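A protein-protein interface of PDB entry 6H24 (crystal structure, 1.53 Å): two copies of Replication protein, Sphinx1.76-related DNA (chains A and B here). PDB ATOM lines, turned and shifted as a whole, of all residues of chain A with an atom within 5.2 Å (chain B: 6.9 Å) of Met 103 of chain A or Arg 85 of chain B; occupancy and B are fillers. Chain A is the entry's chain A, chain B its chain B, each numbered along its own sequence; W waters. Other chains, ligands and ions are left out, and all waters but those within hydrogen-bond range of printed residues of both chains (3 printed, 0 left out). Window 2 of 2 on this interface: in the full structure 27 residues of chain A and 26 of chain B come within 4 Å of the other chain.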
ATOM      1  N   TYR A  64     -18.390  10.317  19.528  1.00  0.00           N
ATOM      2  CA  TYR A  64     -17.541  10.516  18.361  1.00  0.00           C
ATOM      3  C   TYR A  64     -17.935  11.776  17.597  1.00  0.00           C
ATOM      4  O   TYR A  64     -17.079  12.594  17.253  1.00  0.00           O
ATOM      5  CB  TYR A  64     -17.588   9.301  17.444  1.00  0.00           C
ATOM      6  CG  TYR A  64     -16.897   9.539  16.119  1.00  0.00           C
ATOM      7  CD1 TYR A  64     -15.546   9.836  16.064  1.00  0.00           C
ATOM      8  CD2 TYR A  64     -17.604   9.486  14.927  1.00  0.00           C
ATOM      9  CE1 TYR A  64     -14.911  10.060  14.851  1.00  0.00           C
ATOM     10  CE2 TYR A  64     -16.980   9.708  13.709  1.00  0.00           C
ATOM     11  CZ  TYR A  64     -15.631   9.995  13.681  1.00  0.00           C
ATOM     12  OH  TYR A  64     -14.999  10.217  12.479  1.00  0.00           O
ATOM     13  N   GLY A 101      -8.234  15.671  11.613  1.00  0.00           N
ATOM     14  CA  GLY A 101      -8.676  14.552  10.804  1.00  0.00           C
ATOM     15  C   GLY A 101      -9.653  13.702  11.576  1.00  0.00           C
ATOM     16  O   GLY A 101      -9.647  13.679  12.809  1.00  0.00           O
ATOM     17  N   TYR A 102     -10.490  12.988  10.836  1.00  0.00           N
ATOM     18  CA  TYR A 102     -11.426  12.073  11.469  1.00  0.00           C
ATOM     19  C   TYR A 102     -11.564  10.803  10.652  1.00  0.00           C
ATOM     20  O   TYR A 102     -11.522  10.826   9.415  1.00  0.00           O
ATOM     21  CB  TYR A 102     -12.806  12.721  11.659  1.00  0.00           C
ATOM     22  CG  TYR A 102     -13.478  13.105  10.370  1.00  0.00           C
ATOM     23  CD1 TYR A 102     -14.205  12.175   9.645  1.00  0.00           C
ATOM     24  CD2 TYR A 102     -13.409  14.404   9.891  1.00  0.00           C
ATOM     25  CE1 TYR A 102     -14.828  12.522   8.454  1.00  0.00           C
ATOM     26  CE2 TYR A 102     -14.034  14.766   8.714  1.00  0.00           C
ATOM     27  CZ  TYR A 102     -14.739  13.821   7.999  1.00  0.00           C
ATOM     28  OH  TYR A 102     -15.364  14.180   6.823  1.00  0.00           O
ATOM     29  N   MET A 103     -11.766   9.698  11.372  1.00  0.00           N
ATOM     30  CA  MET A 103     -11.992   8.377  10.789  1.00  0.00           C
ATOM     31  C   MET A 103     -13.328   7.846  11.304  1.00  0.00           C
ATOM     32  O   MET A 103     -13.413   7.363  12.440  1.00  0.00           O
ATOM     33  CB  MET A 103     -10.863   7.424  11.150  1.00  0.00           C
ATOM     34  CG  MET A 103      -9.511   7.847  10.640  1.00  0.00           C
ATOM     35  SD  MET A 103      -8.223   6.716  11.184  1.00  0.00           S
ATOM     36  CE  MET A 103      -8.726   5.229  10.327  1.00  0.00           C
ATOM     37  N   ASP A 104     -14.357   7.910  10.465  1.00  0.00           N
ATOM     38  CA  ASP A 104     -15.686   7.483  10.882  1.00  0.00           C
ATOM     39  C   ASP A 104     -15.711   6.013  11.279  1.00  0.00           C
ATOM     40  O   ASP A 104     -16.440   5.628  12.202  1.00  0.00           O
ATOM     41  CB  ASP A 104     -16.681   7.731   9.753  1.00  0.00           C
ATOM     42  CG  ASP A 104     -16.995   9.199   9.563  1.00  0.00           C
ATOM     43  OD1 ASP A 104     -16.617  10.021  10.419  1.00  0.00           O
ATOM     44  OD2 ASP A 104     -17.606   9.533   8.523  1.00  0.00           O
ATOM     45  N   ASP A 105     -14.976   5.163  10.557  1.00  0.00           N
ATOM     46  CA  ASP A 105     -15.107   3.723  10.759  1.00  0.00           C
ATOM     47  C   ASP A 105     -14.520   3.257  12.091  1.00  0.00           C
ATOM     48  O   ASP A 105     -14.918   2.195  12.587  1.00  0.00           O
ATOM     49  CB  ASP A 105     -14.463   2.970   9.593  1.00  0.00           C
ATOM     50  CG  ASP A 105     -15.295   3.050   8.319  1.00  0.00           C
ATOM     51  OD1 ASP A 105     -16.382   3.670   8.350  1.00  0.00           O
ATOM     52  OD2 ASP A 105     -14.864   2.495   7.288  1.00  0.00           O
ATOM     53  N   THR A 106     -13.571   3.999  12.662  1.00  0.00           N
ATOM     54  CA  THR A 106     -12.957   3.640  13.935  1.00  0.00           C
ATOM     55  C   THR A 106     -13.277   4.606  15.070  1.00  0.00           C
ATOM     56  O   THR A 106     -12.747   4.436  16.174  1.00  0.00           O
ATOM     57  CB  THR A 106     -11.432   3.549  13.786  1.00  0.00           C
ATOM     58  OG1 THR A 106     -10.924   4.793  13.285  1.00  0.00           O
ATOM     59  CG2 THR A 106     -11.050   2.424  12.840  1.00  0.00           C
ATOM     60  N   ALA A 107     -14.113   5.611  14.834  1.00  0.00           N
ATOM     61  CA  ALA A 107     -14.476   6.587  15.862  1.00  0.00           C
ATOM     62  C   ALA A 107     -13.235   7.196  16.507  1.00  0.00           C
ATOM     63  O   ALA A 107     -13.104   7.242  17.733  1.00  0.00           O
ATOM     64  CB  ALA A 107     -15.373   5.962  16.928  1.00  0.00           C
ATOM     65  N   THR A 108     -12.327   7.677  15.661  1.00  0.00           N
ATOM     66  CA  THR A 108     -11.106   8.337  16.099  1.00  0.00           C
ATOM     67  C   THR A 108     -10.938   9.648  15.347  1.00  0.00           C
ATOM     68  O   THR A 108     -11.403   9.799  14.209  1.00  0.00           O
ATOM     69  CB  THR A 108      -9.871   7.456  15.870  1.00  0.00           C
ATOM     70  OG1 THR A 108      -9.709   7.205  14.470  1.00  0.00           O
ATOM     71  CG2 THR A 108     -10.025   6.133  16.582  1.00  0.00           C
ATOM     72  N   VAL A 109     -10.276  10.600  15.998  1.00  0.00           N
ATOM     73  CA  VAL A 109      -9.882  11.857  15.382  1.00  0.00           C
ATOM     74  C   VAL A 109      -8.374  12.030  15.570  1.00  0.00           C
ATOM     75  O   VAL A 109      -7.728  11.303  16.328  1.00  0.00           O
ATOM     76  CB  VAL A 109     -10.653  13.063  15.962  1.00  0.00           C
ATOM     77  CG1 VAL A 109     -12.163  12.903  15.731  1.00  0.00           C
ATOM     78  CG2 VAL A 109     -10.349  13.230  17.433  1.00  0.00           C
ATOM     79  N   GLU A 110      -7.814  12.993  14.842  1.00  0.00           N
ATOM     80  CA  GLU A 110      -6.385  13.270  14.854  1.00  0.00           C
ATOM     81  C   GLU A 110      -6.195  14.779  14.830  1.00  0.00           C
ATOM     82  O   GLU A 110      -6.893  15.476  14.094  1.00  0.00           O
ATOM     83  CB  GLU A 110      -5.675  12.680  13.636  1.00  0.00           C
ATOM     84  CG  GLU A 110      -5.333  11.224  13.703  1.00  0.00           C
ATOM     85  CD  GLU A 110      -4.425  10.828  12.559  1.00  0.00           C
ATOM     86  OE1 GLU A 110      -4.000  11.728  11.798  1.00  0.00           O
ATOM     87  OE2 GLU A 110      -4.151   9.625  12.406  1.00  0.00           O
ATOM     88  N   GLN B  82      -7.481  12.876   1.847  1.00  0.00           N
ATOM     89  CA  GLN B  82      -7.702  11.608   2.526  1.00  0.00           C
ATOM     90  C   GLN B  82      -6.428  10.783   2.556  1.00  0.00           C
ATOM     91  O   GLN B  82      -5.536  10.951   1.720  1.00  0.00           O
ATOM     92  CB  GLN B  82      -8.831  10.847   1.830  1.00  0.00           C
ATOM     93  CG  GLN B  82     -10.170  11.559   1.996  1.00  0.00           C
ATOM     94  CD  GLN B  82     -11.251  11.011   1.089  1.00  0.00           C
ATOM     95  OE1 GLN B  82     -10.963  10.451   0.031  1.00  0.00           O
ATOM     96  NE2 GLN B  82     -12.506  11.184   1.491  1.00  0.00           N
ATOM     97  N   GLU B  83      -6.340   9.902   3.547  1.00  0.00           N
ATOM     98  CA  GLU B  83      -5.263   8.934   3.615  1.00  0.00           C
ATOM     99  C   GLU B  83      -5.862   7.582   3.960  1.00  0.00           C
ATOM    100  O   GLU B  83      -6.880   7.496   4.651  1.00  0.00           O
ATOM    101  CB  GLU B  83      -4.226   9.327   4.663  1.00  0.00           C
ATOM    102  CG  GLU B  83      -3.321  10.426   4.187  1.00  0.00           C
ATOM    103  CD  GLU B  83      -2.205  10.731   5.154  1.00  0.00           C
ATOM    104  OE1 GLU B  83      -2.177  10.112   6.241  1.00  0.00           O
ATOM    105  OE2 GLU B  83      -1.375  11.605   4.830  1.00  0.00           O
ATOM    106  N   LYS B  84      -5.231   6.525   3.464  1.00  0.00           N
ATOM    107  CA  LYS B  84      -5.592   5.188   3.901  1.00  0.00           C
ATOM    108  C   LYS B  84      -4.927   4.929   5.246  1.00  0.00           C
ATOM    109  O   LYS B  84      -3.738   5.205   5.431  1.00  0.00           O
ATOM    110  CB  LYS B  84      -5.166   4.145   2.871  1.00  0.00           C
ATOM    111  N   ARG B  85      -5.690   4.370   6.170  1.00  0.00           N
ATOM    112  CA  ARG B  85      -5.182   3.897   7.448  1.00  0.00           C
ATOM    113  C   ARG B  85      -5.466   2.402   7.529  1.00  0.00           C
ATOM    114  O   ARG B  85      -6.119   1.825   6.655  1.00  0.00           O
ATOM    115  CB  ARG B  85      -5.823   4.655   8.620  1.00  0.00           C
ATOM    116  CG  ARG B  85      -5.491   6.170   8.741  1.00  0.00           C
ATOM    117  CD  ARG B  85      -4.240   6.474   9.582  1.00  0.00           C
ATOM    118  NE  ARG B  85      -4.028   7.913   9.782  1.00  0.00           N
ATOM    119  CZ  ARG B  85      -3.424   8.710   8.904  1.00  0.00           C
ATOM    120  NH1 ARG B  85      -2.974   8.212   7.763  1.00  0.00           N
ATOM    121  NH2 ARG B  85      -3.270  10.003   9.160  1.00  0.00           N
ATOM    122  N   GLU B  86      -4.952   1.764   8.582  1.00  0.00           N
ATOM    123  CA  GLU B  86      -5.149   0.328   8.747  1.00  0.00           C
ATOM    124  C   GLU B  86      -6.623  -0.056   8.662  1.00  0.00           C
ATOM    125  O   GLU B  86      -7.002  -0.942   7.885  1.00  0.00           O
ATOM    126  CB  GLU B  86      -4.559  -0.122  10.087  1.00  0.00           C
ATOM    127  N   ARG B  87      -7.468   0.586   9.466  1.00  0.00           N
ATOM    128  CA  ARG B  87      -8.864   0.193   9.598  1.00  0.00           C
ATOM    129  C   ARG B  87      -9.813   0.984   8.705  1.00  0.00           C
ATOM    130  O   ARG B  87     -11.029   0.790   8.801  1.00  0.00           O
ATOM    131  CB  ARG B  87      -9.312   0.328  11.058  1.00  0.00           C
ATOM    132  N   GLY B  88      -9.308   1.862   7.846  1.00  0.00           N
ATOM    133  CA  GLY B  88     -10.189   2.604   6.963  1.00  0.00           C
ATOM    134  C   GLY B  88      -9.533   3.879   6.459  1.00  0.00           C
ATOM    135  O   GLY B  88      -8.312   4.013   6.468  1.00  0.00           O
ATOM    136  N   ARG B  89     -10.386   4.806   6.033  1.00  0.00           N
ATOM    137  CA  ARG B  89      -9.967   6.070   5.449  1.00  0.00           C
ATOM    138  C   ARG B  89     -10.116   7.212   6.444  1.00  0.00           C
ATOM    139  O   ARG B  89     -11.096   7.274   7.193  1.00  0.00           O
ATOM    140  CB  ARG B  89     -10.805   6.358   4.200  1.00  0.00           C
ATOM    141  CG  ARG B  89     -10.383   7.566   3.396  1.00  0.00           C
ATOM    142  CD  ARG B  89     -11.073   7.564   2.037  1.00  0.00           C
ATOM    143  NE  ARG B  89     -12.525   7.694   2.147  1.00  0.00           N
ATOM    144  CZ  ARG B  89     -13.370   7.539   1.130  1.00  0.00           C
ATOM    145  NH1 ARG B  89     -12.914   7.238  -0.077  1.00  0.00           N
ATOM    146  NH2 ARG B  89     -14.675   7.680   1.322  1.00  0.00           N
ATOM    147  N   ILE B  90      -9.143   8.121   6.441  1.00  0.00           N
ATOM    148  CA  ILE B  90      -9.180   9.307   7.284  1.00  0.00           C
ATOM    149  C   ILE B  90      -9.363  10.531   6.392  1.00  0.00           C
ATOM    150  O   ILE B  90      -8.741  10.639   5.327  1.00  0.00           O
ATOM    151  CB  ILE B  90      -7.913   9.445   8.161  1.00  0.00           C
ATOM    152  CG1 ILE B  90      -8.061  10.657   9.090  1.00  0.00           C
ATOM    153  CG2 ILE B  90      -6.647   9.553   7.319  1.00  0.00           C
ATOM    154  CD1 ILE B  90      -7.095  10.676  10.261  1.00  0.00           C
ATOM    155  N   ASN B  91     -10.226  11.445   6.842  1.00  0.00           N
ATOM    156  CA  ASN B  91     -10.486  12.721   6.179  1.00  0.00           C
ATOM    157  C   ASN B  91      -9.731  13.814   6.923  1.00  0.00           C
ATOM    158  O   ASN B  91     -10.049  14.115   8.077  1.00  0.00           O
ATOM    159  CB  ASN B  91     -11.979  13.035   6.142  1.00  0.00           C
ATOM    160  CG  ASN B  91     -12.714  12.237   5.088  1.00  0.00           C
ATOM    161  OD1 ASN B  91     -12.537  12.468   3.896  1.00  0.00           O
ATOM    162  ND2 ASN B  91     -13.545  11.308   5.519  1.00  0.00           N
ATOM    163  N   ILE B  92      -8.725  14.389   6.270  1.00  0.00           N
ATOM    164  CA  ILE B  92      -7.831  15.369   6.884  1.00  0.00           C
ATOM    165  C   ILE B  92      -8.146  16.753   6.333  1.00  0.00           C
ATOM    166  O   ILE B  92      -8.333  16.926   5.123  1.00  0.00           O
ATOM    167  CB  ILE B  92      -6.363  14.997   6.616  1.00  0.00           C
ATOM    168  CG1 ILE B  92      -6.048  13.662   7.296  1.00  0.00           C
ATOM    169  CG2 ILE B  92      -5.418  16.090   7.116  1.00  0.00           C
ATOM    170  CD1 ILE B  92      -4.724  13.064   6.903  1.00  0.00           C
HETATM  171  O   HOH W   1     -13.554   9.005   7.723  1.00  0.00           O
HETATM  172  O   HOH W   2     -13.213   4.332   5.791  1.00  0.00           O
HETATM  173  O   HOH W   3     -13.021   5.548   8.321  1.00  0.00           O
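Water W3 lies within hydrogen-bond range of O of Arg 89 of chain B (2.8 Å), N of Asp 105 of chain A (3.0 Å) and N of Asp 104 of chain A (3.5 Å). Water W2 bridges N of Arg 89 of chain B (2.9 Å) and OD2 of Asp 105 of chain A (2.9 Å). Water W1 lies within hydrogen-bond range of the backbone carbonyl oxygen of Arg 89 of chain B (3.1 Å), the backbone NH of Asp 104 of chain A (3.1 Å), the side-chain amide nitrogen of Asn 91 of chain B (3.2 Å) and the backbone carbonyl oxygen of Tyr 102 of chain A (3.2 Å).
No position is printed for both chains. Of the 9 pairs that touch across the chains among the printed residues, none has its exchanged pair printed and touching as well.
N of Asn 91 of chain B lies within hydrogen-bond range of O of Tyr 102 of chain A (2.9 Å). OE2 of Glu 110 of chain A lies within salt-bridge range of NE of Arg 85 of chain B (3.1 Å).
Of the printed residues of chain B, Met 103 of chain A touches Arg 85, Arg 89 and Ile 90. Of the printed residues of chain B, Thr 106 of chain A touches Arg 87 (3.3 Å). Lys 84 of chain B touches none of the printed residues of chain A. Printed residues of chain A within 4 Å of Arg 85 of chain B: Met 103 and Glu 110. Of the printed residues of chain A, Arg 87 of chain B touches Thr 106. Gly 88 of chain B touches none of the printed residues of chain A. Of the printed residues of chain A, Asn 91 of chain B touches Gly 101 and Tyr 102.
N of Glu 110 of chain A is in hydrogen-bond range of O of Gly 101 of chain A. The backbone NH of Met 103 of chain A is in hydrogen-bond range of the backbone carbonyl oxygen of Thr 108 of chain A, at 2.9 Å. The side-chain hydroxyl (OG1) of Thr 106 of chain A lies within hydrogen-bond range of the side-chain hydroxyl (OG1) of Thr 108 of chain A (2.9 Å). The side-chain amide nitrogen (NE2) of Gln 82 of chain B sits at hydrogen-bond distance from the side-chain amide oxygen (OD1) of Asn 91 of chain B, 2.7 Å away. The guanidinium group (NH1) of Arg 85 of chain B is in salt-bridge range of the side-chain carboxylate (OE1) of Glu 83 of chain B (2.6 Å). N of Ile 90 of chain B sits at hydrogen-bond distance from O of Glu 83 of chain B (3.0 Å).
Hydrophobic or aromatic side chains of chain B within 4 Å of the printed part of chain A: Ile 90. Along chain B the printed residues that touch a printed residue of chain A span positions 85 to 91. Hydrophobic or aromatic side chains of chain A that line the printed part of chain B: Tyr 102 and Met 103. Along chain A the printed residues that touch a printed residue of chain B span positions 101 to 110. Among the printed residues, Asp or Glu carboxylates within 4 Å of a Lys or Arg side-chain nitrogen of the other chain: Glu 110 of chain A with Arg 85 of chain B.
Among the printed residues, merely in contact across the chains: Gly 101 of chain A with Asn 91 of chain B (3.1 Å), Tyr 102 of chain A with Ile 90 of chain B (3.5 Å), Met 103 of chain A with Arg 85 of chain B (3.4 Å), Met 103 of chain A with Arg 89 of chain B (3.8 Å), Met 103 of chain A with Ile 90 of chain B (3.4 Å), Thr 106 of chain A with Arg 87 of chain B (3.3 Å) and Glu 110 of chain A with Ile 90 of chain B (3.5 Å).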
